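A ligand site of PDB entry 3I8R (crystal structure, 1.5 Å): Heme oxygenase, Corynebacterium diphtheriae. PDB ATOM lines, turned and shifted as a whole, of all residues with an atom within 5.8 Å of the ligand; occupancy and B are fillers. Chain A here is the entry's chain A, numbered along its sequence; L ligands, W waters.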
ATOM      1  N   ALA A   9       7.845 -12.841   1.678  1.00  0.00           N
ATOM      2  CA  ALA A   9       8.917 -12.897   2.730  1.00  0.00           C
ATOM      3  C   ALA A   9      10.270 -12.454   2.172  1.00  0.00           C
ATOM      4  O   ALA A   9      11.046 -11.692   2.789  1.00  0.00           O
ATOM      5  CB  ALA A   9       8.995 -14.316   3.330  1.00  0.00           C
ATOM      6  N   LEU A  12      10.070  -8.584   1.440  1.00  0.00           N
ATOM      7  CA  LEU A  12      10.244  -7.882   2.739  1.00  0.00           C
ATOM      8  C   LEU A  12      11.715  -7.766   3.211  1.00  0.00           C
ATOM      9  O   LEU A  12      12.155  -6.607   3.467  1.00  0.00           O
ATOM     10  CB  LEU A  12       9.388  -8.575   3.793  1.00  0.00           C
ATOM     11  CG  LEU A  12       7.877  -8.045   3.810  1.00  0.00           C
ATOM     12  CD1 LEU A  12       7.089  -9.000   4.630  1.00  0.00           C
ATOM     13  CD2 LEU A  12       7.888  -6.617   4.364  1.00  0.00           C
ATOM     14  N   LYS A  13      12.431  -8.926   3.188  1.00  0.00           N
ATOM     15  CA  LYS A  13      13.775  -8.982   3.681  1.00  0.00           C
ATOM     16  C   LYS A  13      14.614  -8.140   2.779  1.00  0.00           C
ATOM     17  O   LYS A  13      15.432  -7.298   3.191  1.00  0.00           O
ATOM     18  CB  LYS A  13      14.259 -10.444   3.715  1.00  0.00           C
ATOM     19  CG  LYS A  13      15.597 -10.599   4.499  1.00  0.00           C
ATOM     20  CD  LYS A  13      16.039 -12.094   4.634  1.00  0.00           C
ATOM     21  CE  LYS A  13      17.365 -12.147   5.422  1.00  0.00           C
ATOM     22  NZ  LYS A  13      18.003 -13.481   5.139  1.00  0.00           N
ATOM     23  N   HIS A  20      18.094  -2.335   7.834  1.00  0.00           N
ATOM     24  CA  HIS A  20      18.511  -3.224   8.923  1.00  0.00           C
ATOM     25  C   HIS A  20      20.031  -3.025   9.227  1.00  0.00           C
ATOM     26  O   HIS A  20      20.417  -2.809  10.379  1.00  0.00           O
ATOM     27  CB  HIS A  20      18.226  -4.665   8.623  1.00  0.00           C
ATOM     28  CG  HIS A  20      18.466  -5.582   9.771  1.00  0.00           C
ATOM     29  ND1 HIS A  20      19.737  -6.024  10.153  1.00  0.00           N
ATOM     30  CD2 HIS A  20      17.600  -6.085  10.678  1.00  0.00           C
ATOM     31  CE1 HIS A  20      19.587  -6.789  11.232  1.00  0.00           C
ATOM     32  NE2 HIS A  20      18.296  -6.876  11.562  1.00  0.00           N
ATOM     33  N   ALA A  23      20.452   0.122  11.131  1.00  0.00           N
ATOM     34  CA  ALA A  23      19.967  -0.008  12.529  1.00  0.00           C
ATOM     35  C   ALA A  23      21.111  -0.682  13.350  1.00  0.00           C
ATOM     36  O   ALA A  23      21.280  -0.294  14.513  1.00  0.00           O
ATOM     37  CB  ALA A  23      18.750  -0.908  12.573  1.00  0.00           C
ATOM     38  N   GLU A  24      21.788  -1.634  12.755  1.00  0.00           N
ATOM     39  CA  GLU A  24      23.011  -2.281  13.389  1.00  0.00           C
ATOM     40  C   GLU A  24      24.035  -1.234  13.801  1.00  0.00           C
ATOM     41  O   GLU A  24      24.774  -1.363  14.813  1.00  0.00           O
ATOM     42  CB  GLU A  24      23.596  -3.359  12.470  1.00  0.00           C
ATOM     43  CG  GLU A  24      22.677  -4.591  12.301  1.00  0.00           C
ATOM     44  CD  GLU A  24      23.307  -5.823  11.625  1.00  0.00           C
ATOM     45  OE1 GLU A  24      24.501  -5.822  11.248  1.00  0.00           O
ATOM     46  OE2 GLU A  24      22.607  -6.863  11.469  1.00  0.00           O
ATOM     47  N   MET A  29      22.497   1.517  19.889  1.00  0.00           N
ATOM     48  CA  MET A  29      22.380   0.058  19.899  1.00  0.00           C
ATOM     49  C   MET A  29      23.779  -0.569  19.738  1.00  0.00           C
ATOM     50  O   MET A  29      24.069  -1.608  20.380  1.00  0.00           O
ATOM     51  CB  MET A  29      21.339  -0.476  18.801  1.00  0.00           C
ATOM     52  CG  MET A  29      20.938  -1.957  19.098  1.00  0.00           C
ATOM     53  SD  MET A  29      20.111  -2.073  20.689  1.00  0.00           S
ATOM     54  CE  MET A  29      19.537  -3.773  20.585  1.00  0.00           C
ATOM     55  N   LEU A  33      25.301  -3.134  22.494  1.00  0.00           N
ATOM     56  CA  LEU A  33      25.660  -4.535  22.207  1.00  0.00           C
ATOM     57  C   LEU A  33      27.148  -4.812  22.333  1.00  0.00           C
ATOM     58  O   LEU A  33      27.534  -5.965  22.532  1.00  0.00           O
ATOM     59  CB  LEU A  33      25.177  -4.900  20.790  1.00  0.00           C
ATOM     60  CG  LEU A  33      23.659  -4.812  20.632  1.00  0.00           C
ATOM     61  CD1 LEU A  33      23.307  -5.218  19.177  1.00  0.00           C
ATOM     62  CD2 LEU A  33      22.891  -5.586  21.541  1.00  0.00           C
ATOM     63  N   TYR A 130       5.855  -8.176  11.094  1.00  0.00           N
ATOM     64  CA  TYR A 130       7.092  -8.733  10.554  1.00  0.00           C
ATOM     65  C   TYR A 130       8.229  -7.939  11.131  1.00  0.00           C
ATOM     66  O   TYR A 130       9.218  -8.588  11.665  1.00  0.00           O
ATOM     67  CB  TYR A 130       7.037  -8.579   9.007  1.00  0.00           C
ATOM     68  CG  TYR A 130       8.404  -8.709   8.357  1.00  0.00           C
ATOM     69  CD1 TYR A 130       8.912  -9.944   8.148  1.00  0.00           C
ATOM     70  CD2 TYR A 130       9.099  -7.589   7.999  1.00  0.00           C
ATOM     71  CE1 TYR A 130      10.172 -10.028   7.605  1.00  0.00           C
ATOM     72  CE2 TYR A 130      10.452  -7.681   7.388  1.00  0.00           C
ATOM     73  CZ  TYR A 130      10.849  -8.924   7.195  1.00  0.00           C
ATOM     74  OH  TYR A 130      12.158  -9.098   6.716  1.00  0.00           O
ATOM     75  N   VAL A 131       8.237  -6.629  11.065  1.00  0.00           N
ATOM     76  CA  VAL A 131       9.468  -5.876  11.481  1.00  0.00           C
ATOM     77  C   VAL A 131       9.794  -6.177  12.921  1.00  0.00           C
ATOM     78  O   VAL A 131      10.991  -6.337  13.275  1.00  0.00           O
ATOM     79  CB  VAL A 131       9.291  -4.406  11.192  1.00  0.00           C
ATOM     80  CG1 VAL A 131      10.464  -3.565  11.810  1.00  0.00           C
ATOM     81  CG2 VAL A 131       9.313  -4.214   9.633  1.00  0.00           C
ATOM     82  N   ARG A 132       8.807  -6.210  13.817  1.00  0.00           N
ATOM     83  CA  ARG A 132       9.122  -6.473  15.211  1.00  0.00           C
ATOM     84  C   ARG A 132       9.247  -7.966  15.478  1.00  0.00           C
ATOM     85  O   ARG A 132      10.344  -8.363  15.997  1.00  0.00           O
ATOM     86  CB  ARG A 132       8.029  -5.877  16.187  1.00  0.00           C
ATOM     87  CG  ARG A 132       8.172  -4.321  16.310  1.00  0.00           C
ATOM     88  CD  ARG A 132       9.670  -3.850  16.601  1.00  0.00           C
ATOM     89  NE  ARG A 132      10.255  -4.651  17.645  1.00  0.00           N
ATOM     90  CZ  ARG A 132      11.441  -4.365  18.158  1.00  0.00           C
ATOM     91  NH1 ARG A 132      12.126  -3.266  17.862  1.00  0.00           N
ATOM     92  NH2 ARG A 132      12.039  -5.257  18.976  1.00  0.00           N
ATOM     93  N   LEU A 134       9.436 -10.850  13.728  1.00  0.00           N
ATOM     94  CA  LEU A 134      10.416 -11.813  13.095  1.00  0.00           C
ATOM     95  C   LEU A 134      11.746 -11.380  13.569  1.00  0.00           C
ATOM     96  O   LEU A 134      12.644 -12.302  13.669  1.00  0.00           O
ATOM     97  CB  LEU A 134      10.250 -11.918  11.584  1.00  0.00           C
ATOM     98  CG  LEU A 134      10.972 -13.128  10.942  1.00  0.00           C
ATOM     99  CD1 LEU A 134      10.518 -14.386  11.603  1.00  0.00           C
ATOM    100  CD2 LEU A 134      10.677 -13.159   9.476  1.00  0.00           C
ATOM    101  N   GLY A 135      12.007 -10.090  13.800  1.00  0.00           N
ATOM    102  CA  GLY A 135      13.347  -9.658  14.318  1.00  0.00           C
ATOM    103  C   GLY A 135      13.518 -10.260  15.662  1.00  0.00           C
ATOM    104  O   GLY A 135      14.596 -10.910  15.977  1.00  0.00           O
ATOM    105  N   ASP A 136      12.554 -10.201  16.570  1.00  0.00           N
ATOM    106  CA  ASP A 136      12.735 -10.736  17.915  1.00  0.00           C
ATOM    107  C   ASP A 136      13.046 -12.237  17.833  1.00  0.00           C
ATOM    108  O   ASP A 136      13.920 -12.714  18.588  1.00  0.00           O
ATOM    109  CB  ASP A 136      11.413 -10.618  18.735  1.00  0.00           C
ATOM    110  CG  ASP A 136      10.987  -9.124  18.918  1.00  0.00           C
ATOM    111  OD1 ASP A 136       9.756  -9.020  19.128  1.00  0.00           O
ATOM    112  OD2 ASP A 136      11.830  -8.242  18.927  1.00  0.00           O
ATOM    113  N   SER A 138      14.354 -13.890  15.425  1.00  0.00           N
ATOM    114  CA  SER A 138      15.600 -14.084  14.594  1.00  0.00           C
ATOM    115  C   SER A 138      16.901 -13.555  15.134  1.00  0.00           C
ATOM    116  O   SER A 138      17.882 -14.367  15.046  1.00  0.00           O
ATOM    117  CB  SER A 138      15.452 -13.430  13.214  1.00  0.00           C
ATOM    118  OG  SER A 138      14.363 -14.055  12.579  1.00  0.00           O
ATOM    119  N   GLY A 139      17.062 -12.261  15.420  1.00  0.00           N
ATOM    120  CA  GLY A 139      18.258 -11.739  16.106  1.00  0.00           C
ATOM    121  C   GLY A 139      18.116 -11.720  17.634  1.00  0.00           C
ATOM    122  O   GLY A 139      19.080 -11.322  18.328  1.00  0.00           O
ATOM    123  N   VAL A 142      20.686 -13.244  19.976  1.00  0.00           N
ATOM    124  CA  VAL A 142      21.950 -12.543  19.969  1.00  0.00           C
ATOM    125  C   VAL A 142      21.856 -11.468  21.017  1.00  0.00           C
ATOM    126  O   VAL A 142      22.779 -11.251  21.843  1.00  0.00           O
ATOM    127  CB  VAL A 142      22.352 -12.036  18.531  1.00  0.00           C
ATOM    128  CG1 VAL A 142      23.486 -11.036  18.608  1.00  0.00           C
ATOM    129  CG2 VAL A 142      22.498 -13.243  17.582  1.00  0.00           C
ATOM    130  N   ILE A 143      20.771 -10.679  20.977  1.00  0.00           N
ATOM    131  CA  ILE A 143      20.625  -9.635  21.938  1.00  0.00           C
ATOM    132  C   ILE A 143      20.562 -10.181  23.384  1.00  0.00           C
ATOM    133  O   ILE A 143      21.274  -9.675  24.252  1.00  0.00           O
ATOM    134  CB  ILE A 143      19.299  -8.879  21.711  1.00  0.00           C
ATOM    135  CG1 ILE A 143      19.172  -8.490  20.216  1.00  0.00           C
ATOM    136  CG2 ILE A 143      19.305  -7.596  22.636  1.00  0.00           C
ATOM    137  CD1 ILE A 143      20.265  -7.564  19.733  1.00  0.00           C
ATOM    138  N   ARG A 177       7.348 -17.386   7.757  1.00  0.00           N
ATOM    139  CA  ARG A 177       7.619 -16.849   6.411  1.00  0.00           C
ATOM    140  C   ARG A 177       6.736 -17.504   5.314  1.00  0.00           C
ATOM    141  O   ARG A 177       6.355 -16.852   4.362  1.00  0.00           O
ATOM    142  CB  ARG A 177       9.079 -17.033   5.966  1.00  0.00           C
ATOM    143  CG  ARG A 177      10.078 -16.148   6.698  1.00  0.00           C
ATOM    144  CD  ARG A 177      11.514 -16.340   6.159  1.00  0.00           C
ATOM    145  NE  ARG A 177      12.438 -15.712   7.073  1.00  0.00           N
ATOM    146  CZ  ARG A 177      12.988 -16.352   8.126  1.00  0.00           C
ATOM    147  NH1 ARG A 177      12.772 -17.683   8.326  1.00  0.00           N
ATOM    148  NH2 ARG A 177      13.737 -15.680   8.985  1.00  0.00           N
ATOM    149  N   ALA A 200       8.283   1.236   9.409  1.00  0.00           N
ATOM    150  CA  ALA A 200       8.499   0.521  10.708  1.00  0.00           C
ATOM    151  C   ALA A 200      10.017   0.535  11.131  1.00  0.00           C
ATOM    152  O   ALA A 200      10.341   0.842  12.236  1.00  0.00           O
ATOM    153  CB  ALA A 200       7.902  -0.842  10.667  1.00  0.00           C
ATOM    154  N   PHE A 201      10.877   0.348  10.118  1.00  0.00           N
ATOM    155  CA  PHE A 201      12.287   0.427  10.467  1.00  0.00           C
ATOM    156  C   PHE A 201      12.714   1.828  10.798  1.00  0.00           C
ATOM    157  O   PHE A 201      13.508   2.050  11.690  1.00  0.00           O
ATOM    158  CB  PHE A 201      13.175  -0.050   9.275  1.00  0.00           C
ATOM    159  CG  PHE A 201      13.534  -1.499   9.378  1.00  0.00           C
ATOM    160  CD1 PHE A 201      12.776  -2.504   8.768  1.00  0.00           C
ATOM    161  CD2 PHE A 201      14.706  -1.852  10.094  1.00  0.00           C
ATOM    162  CE1 PHE A 201      13.006  -3.882   8.892  1.00  0.00           C
ATOM    163  CE2 PHE A 201      15.041  -3.235  10.243  1.00  0.00           C
ATOM    164  CZ  PHE A 201      14.200  -4.319   9.635  1.00  0.00           C
ATOM    165  N   ASN A 204      11.685   2.512  14.397  1.00  0.00           N
ATOM    166  CA  ASN A 204      12.611   1.799  15.296  1.00  0.00           C
ATOM    167  C   ASN A 204      13.972   2.444  15.383  1.00  0.00           C
ATOM    168  O   ASN A 204      14.571   2.460  16.485  1.00  0.00           O
ATOM    169  CB  ASN A 204      12.642   0.344  14.893  1.00  0.00           C
ATOM    170  CG  ASN A 204      11.494  -0.437  15.502  1.00  0.00           C
ATOM    171  OD1 ASN A 204      11.518  -0.723  16.717  1.00  0.00           O
ATOM    172  ND2 ASN A 204      10.426  -0.709  14.699  1.00  0.00           N
ATOM    173  N   HIS A 205      14.476   2.848  14.225  1.00  0.00           N
ATOM    174  CA  HIS A 205      15.834   3.477  14.268  1.00  0.00           C
ATOM    175  C   HIS A 205      15.775   4.773  15.100  1.00  0.00           C
ATOM    176  O   HIS A 205      16.633   5.087  15.895  1.00  0.00           O
ATOM    177  CB  HIS A 205      16.349   3.644  12.859  1.00  0.00           C
ATOM    178  CG  HIS A 205      17.803   4.029  12.788  1.00  0.00           C
ATOM    179  ND1 HIS A 205      18.562   3.633  11.706  1.00  0.00           N
ATOM    180  CD2 HIS A 205      18.624   4.711  13.620  1.00  0.00           C
ATOM    181  CE1 HIS A 205      19.774   4.161  11.827  1.00  0.00           C
ATOM    182  NE2 HIS A 205      19.818   4.846  12.963  1.00  0.00           N
ATOM    183  N   PHE A 208      16.080   4.325  18.833  1.00  0.00           N
ATOM    184  CA  PHE A 208      17.470   4.212  19.290  1.00  0.00           C
ATOM    185  C   PHE A 208      18.112   5.591  19.293  1.00  0.00           C
ATOM    186  O   PHE A 208      18.875   5.870  20.203  1.00  0.00           O
ATOM    187  CB  PHE A 208      18.302   3.344  18.338  1.00  0.00           C
ATOM    188  CG  PHE A 208      17.901   1.913  18.270  1.00  0.00           C
ATOM    189  CD1 PHE A 208      17.215   1.263  19.239  1.00  0.00           C
ATOM    190  CD2 PHE A 208      18.299   1.200  17.131  1.00  0.00           C
ATOM    191  CE1 PHE A 208      16.946  -0.139  19.137  1.00  0.00           C
ATOM    192  CE2 PHE A 208      18.081  -0.182  16.977  1.00  0.00           C
ATOM    193  CZ  PHE A 208      17.354  -0.841  17.989  1.00  0.00           C
HETATM  194  C1  LIG L   1      16.983 -10.480  11.413  1.00  0.00           C
HETATM  195  C2  LIG L   1      14.319  -6.485  12.551  1.00  0.00           C
HETATM  196  C3  LIG L   1      18.320  -4.600  14.676  1.00  0.00           C
HETATM  197  C4  LIG L   1      20.589  -8.876  14.364  1.00  0.00           C
HETATM  198  C5  LIG L   1      15.967  -9.524  11.548  1.00  0.00           C
HETATM  199  C6  LIG L   1      14.658  -9.716  10.886  1.00  0.00           C
HETATM  200  C7  LIG L   1      13.939  -8.641  11.220  1.00  0.00           C
HETATM  201  C8  LIG L   1      14.725  -7.700  12.000  1.00  0.00           C
HETATM  202  C9  LIG L   1      12.520  -8.325  10.807  1.00  0.00           C
HETATM  203  C10 LIG L   1      14.274 -10.959  10.085  1.00  0.00           C
HETATM  204  C11 LIG L   1      14.589 -10.671   8.615  1.00  0.00           C
HETATM  205  C12 LIG L   1      13.976 -11.782   7.732  1.00  0.00           C
HETATM  206  O1  LIG L   1      14.252 -13.055   7.952  1.00  0.00           O
HETATM  207  O2  LIG L   1      13.113 -11.494   6.815  1.00  0.00           O
HETATM  208  C13 LIG L   1      15.115  -5.618  13.212  1.00  0.00           C
HETATM  209  C14 LIG L   1      14.913  -4.334  13.660  1.00  0.00           C
HETATM  210  C15 LIG L   1      15.994  -3.714  14.258  1.00  0.00           C
HETATM  211  C16 LIG L   1      17.034  -4.796  14.161  1.00  0.00           C
HETATM  212  C17 LIG L   1      13.517  -3.644  13.474  1.00  0.00           C
HETATM  213  C18 LIG L   1      16.228  -2.304  14.831  1.00  0.00           C
HETATM  214  C19 LIG L   1      15.746  -1.187  14.220  1.00  0.00           C
HETATM  215  C20 LIG L   1      19.251  -5.602  14.779  1.00  0.00           C
HETATM  216  C21 LIG L   1      20.532  -5.426  15.487  1.00  0.00           C
HETATM  217  C22 LIG L   1      21.114  -6.607  15.395  1.00  0.00           C
HETATM  218  C23 LIG L   1      20.338  -7.550  14.636  1.00  0.00           C
HETATM  219  C24 LIG L   1      21.059  -4.170  16.194  1.00  0.00           C
HETATM  220  C25 LIG L   1      22.486  -6.937  15.982  1.00  0.00           C
HETATM  221  C26 LIG L   1      22.495  -8.001  16.800  1.00  0.00           C
HETATM  222  C27 LIG L   1      19.853  -9.619  13.483  1.00  0.00           C
HETATM  223  C28 LIG L   1      20.312 -10.770  12.834  1.00  0.00           C
HETATM  224  C29 LIG L   1      19.249 -11.270  11.906  1.00  0.00           C
HETATM  225  C30 LIG L   1      18.147 -10.352  12.151  1.00  0.00           C
HETATM  226  C31 LIG L   1      21.667 -11.406  13.112  1.00  0.00           C
HETATM  227  C32 LIG L   1      19.339 -12.506  10.956  1.00  0.00           C
HETATM  228  C33 LIG L   1      19.734 -11.774   9.594  1.00  0.00           C
HETATM  229  C34 LIG L   1      20.877 -10.697   9.400  1.00  0.00           C
HETATM  230  O3  LIG L   1      20.758  -9.565   8.811  1.00  0.00           O
HETATM  231  O4  LIG L   1      22.060 -10.914   9.762  1.00  0.00           O
HETATM  232  N1  LIG L   1      15.977  -8.319  12.198  1.00  0.00           N
HETATM  233  N2  LIG L   1      16.450  -5.921  13.585  1.00  0.00           N
HETATM  234  N3  LIG L   1      19.117  -6.890  14.332  1.00  0.00           N
HETATM  235  N4  LIG L   1      18.579  -9.353  12.926  1.00  0.00           N
HETATM  236 FE1  LIG L   1      17.580  -7.613  13.244  1.00  0.00          FE
HETATM  237  O   HOH W   1      11.911 -13.177   5.263  1.00  0.00           O
HETATM  238  O   HOH W   2      16.608 -13.689   9.122  1.00  0.00           O
HETATM  239  O   HOH W   3      19.924 -13.153   6.611  1.00  0.00           O
HETATM  240  O   HOH W   4      15.362 -14.902   6.147  1.00  0.00           O
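Water W1 lies within hydrogen-bond range of an oxygen (O2) of the ligand, the backbone carbonyl oxygen (O) of Ala 9 and the guanidinium group (NE) of Arg 177. Water W2 bridges O1 of the ligand (2.7 Å) and NH2 of Arg 177 (3.5 Å). Water W4 lies within hydrogen-bond range of O1 of the ligand, NZ of Lys 13 and NE of Arg 177.
An iron atom (FE1) of the ligand is bound by a ring nitrogen (NE2) of His 20 (2.0 Å). The side-chain hydroxyl (OH) of Tyr 130 lies within hydrogen-bond range of an oxygen (O2) of the ligand, 2.6 Å away. The guanidinium group (NH2) of Arg 177 lies within salt-bridge range of an oxygen (O1) of the ligand (2.9 Å).
ND1 of His 20 lies close to OE2 of Glu 24. The side-chain amide oxygen of Asn 204 sits at hydrogen-bond distance from the guanidinium group of Arg 132 (2.9 Å). The side-chain amide nitrogen of Asn 204 sits at hydrogen-bond distance from the backbone carbonyl oxygen of Ala 200. The side-chain hydroxyl (OG) of Ser 138 lies within hydrogen-bond range of the backbone carbonyl oxygen (O) of Leu 134, at 2.7 Å.
Residues that only touch the ligand: Gly 135, Val 131, Ala 23, Lys 13, Asn 204, Phe 208, Phe 201, Met 29, Val 142, Ile 143, Leu 33, Gly 139, Ser 138, Leu 134 and Glu 24. Hydrophobic or aromatic side chains within 4 Å of the ligand: His 20, Ala 23, Met 29, Leu 33, Tyr 130, Val 131, Leu 134, Val 142, Ile 143, Phe 201 and Phe 208. Of the 24 residues printed, 18 come within 4 Å of the ligand. The nearest printed residue that does not touch the ligand is His 205 (4.2 Å).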
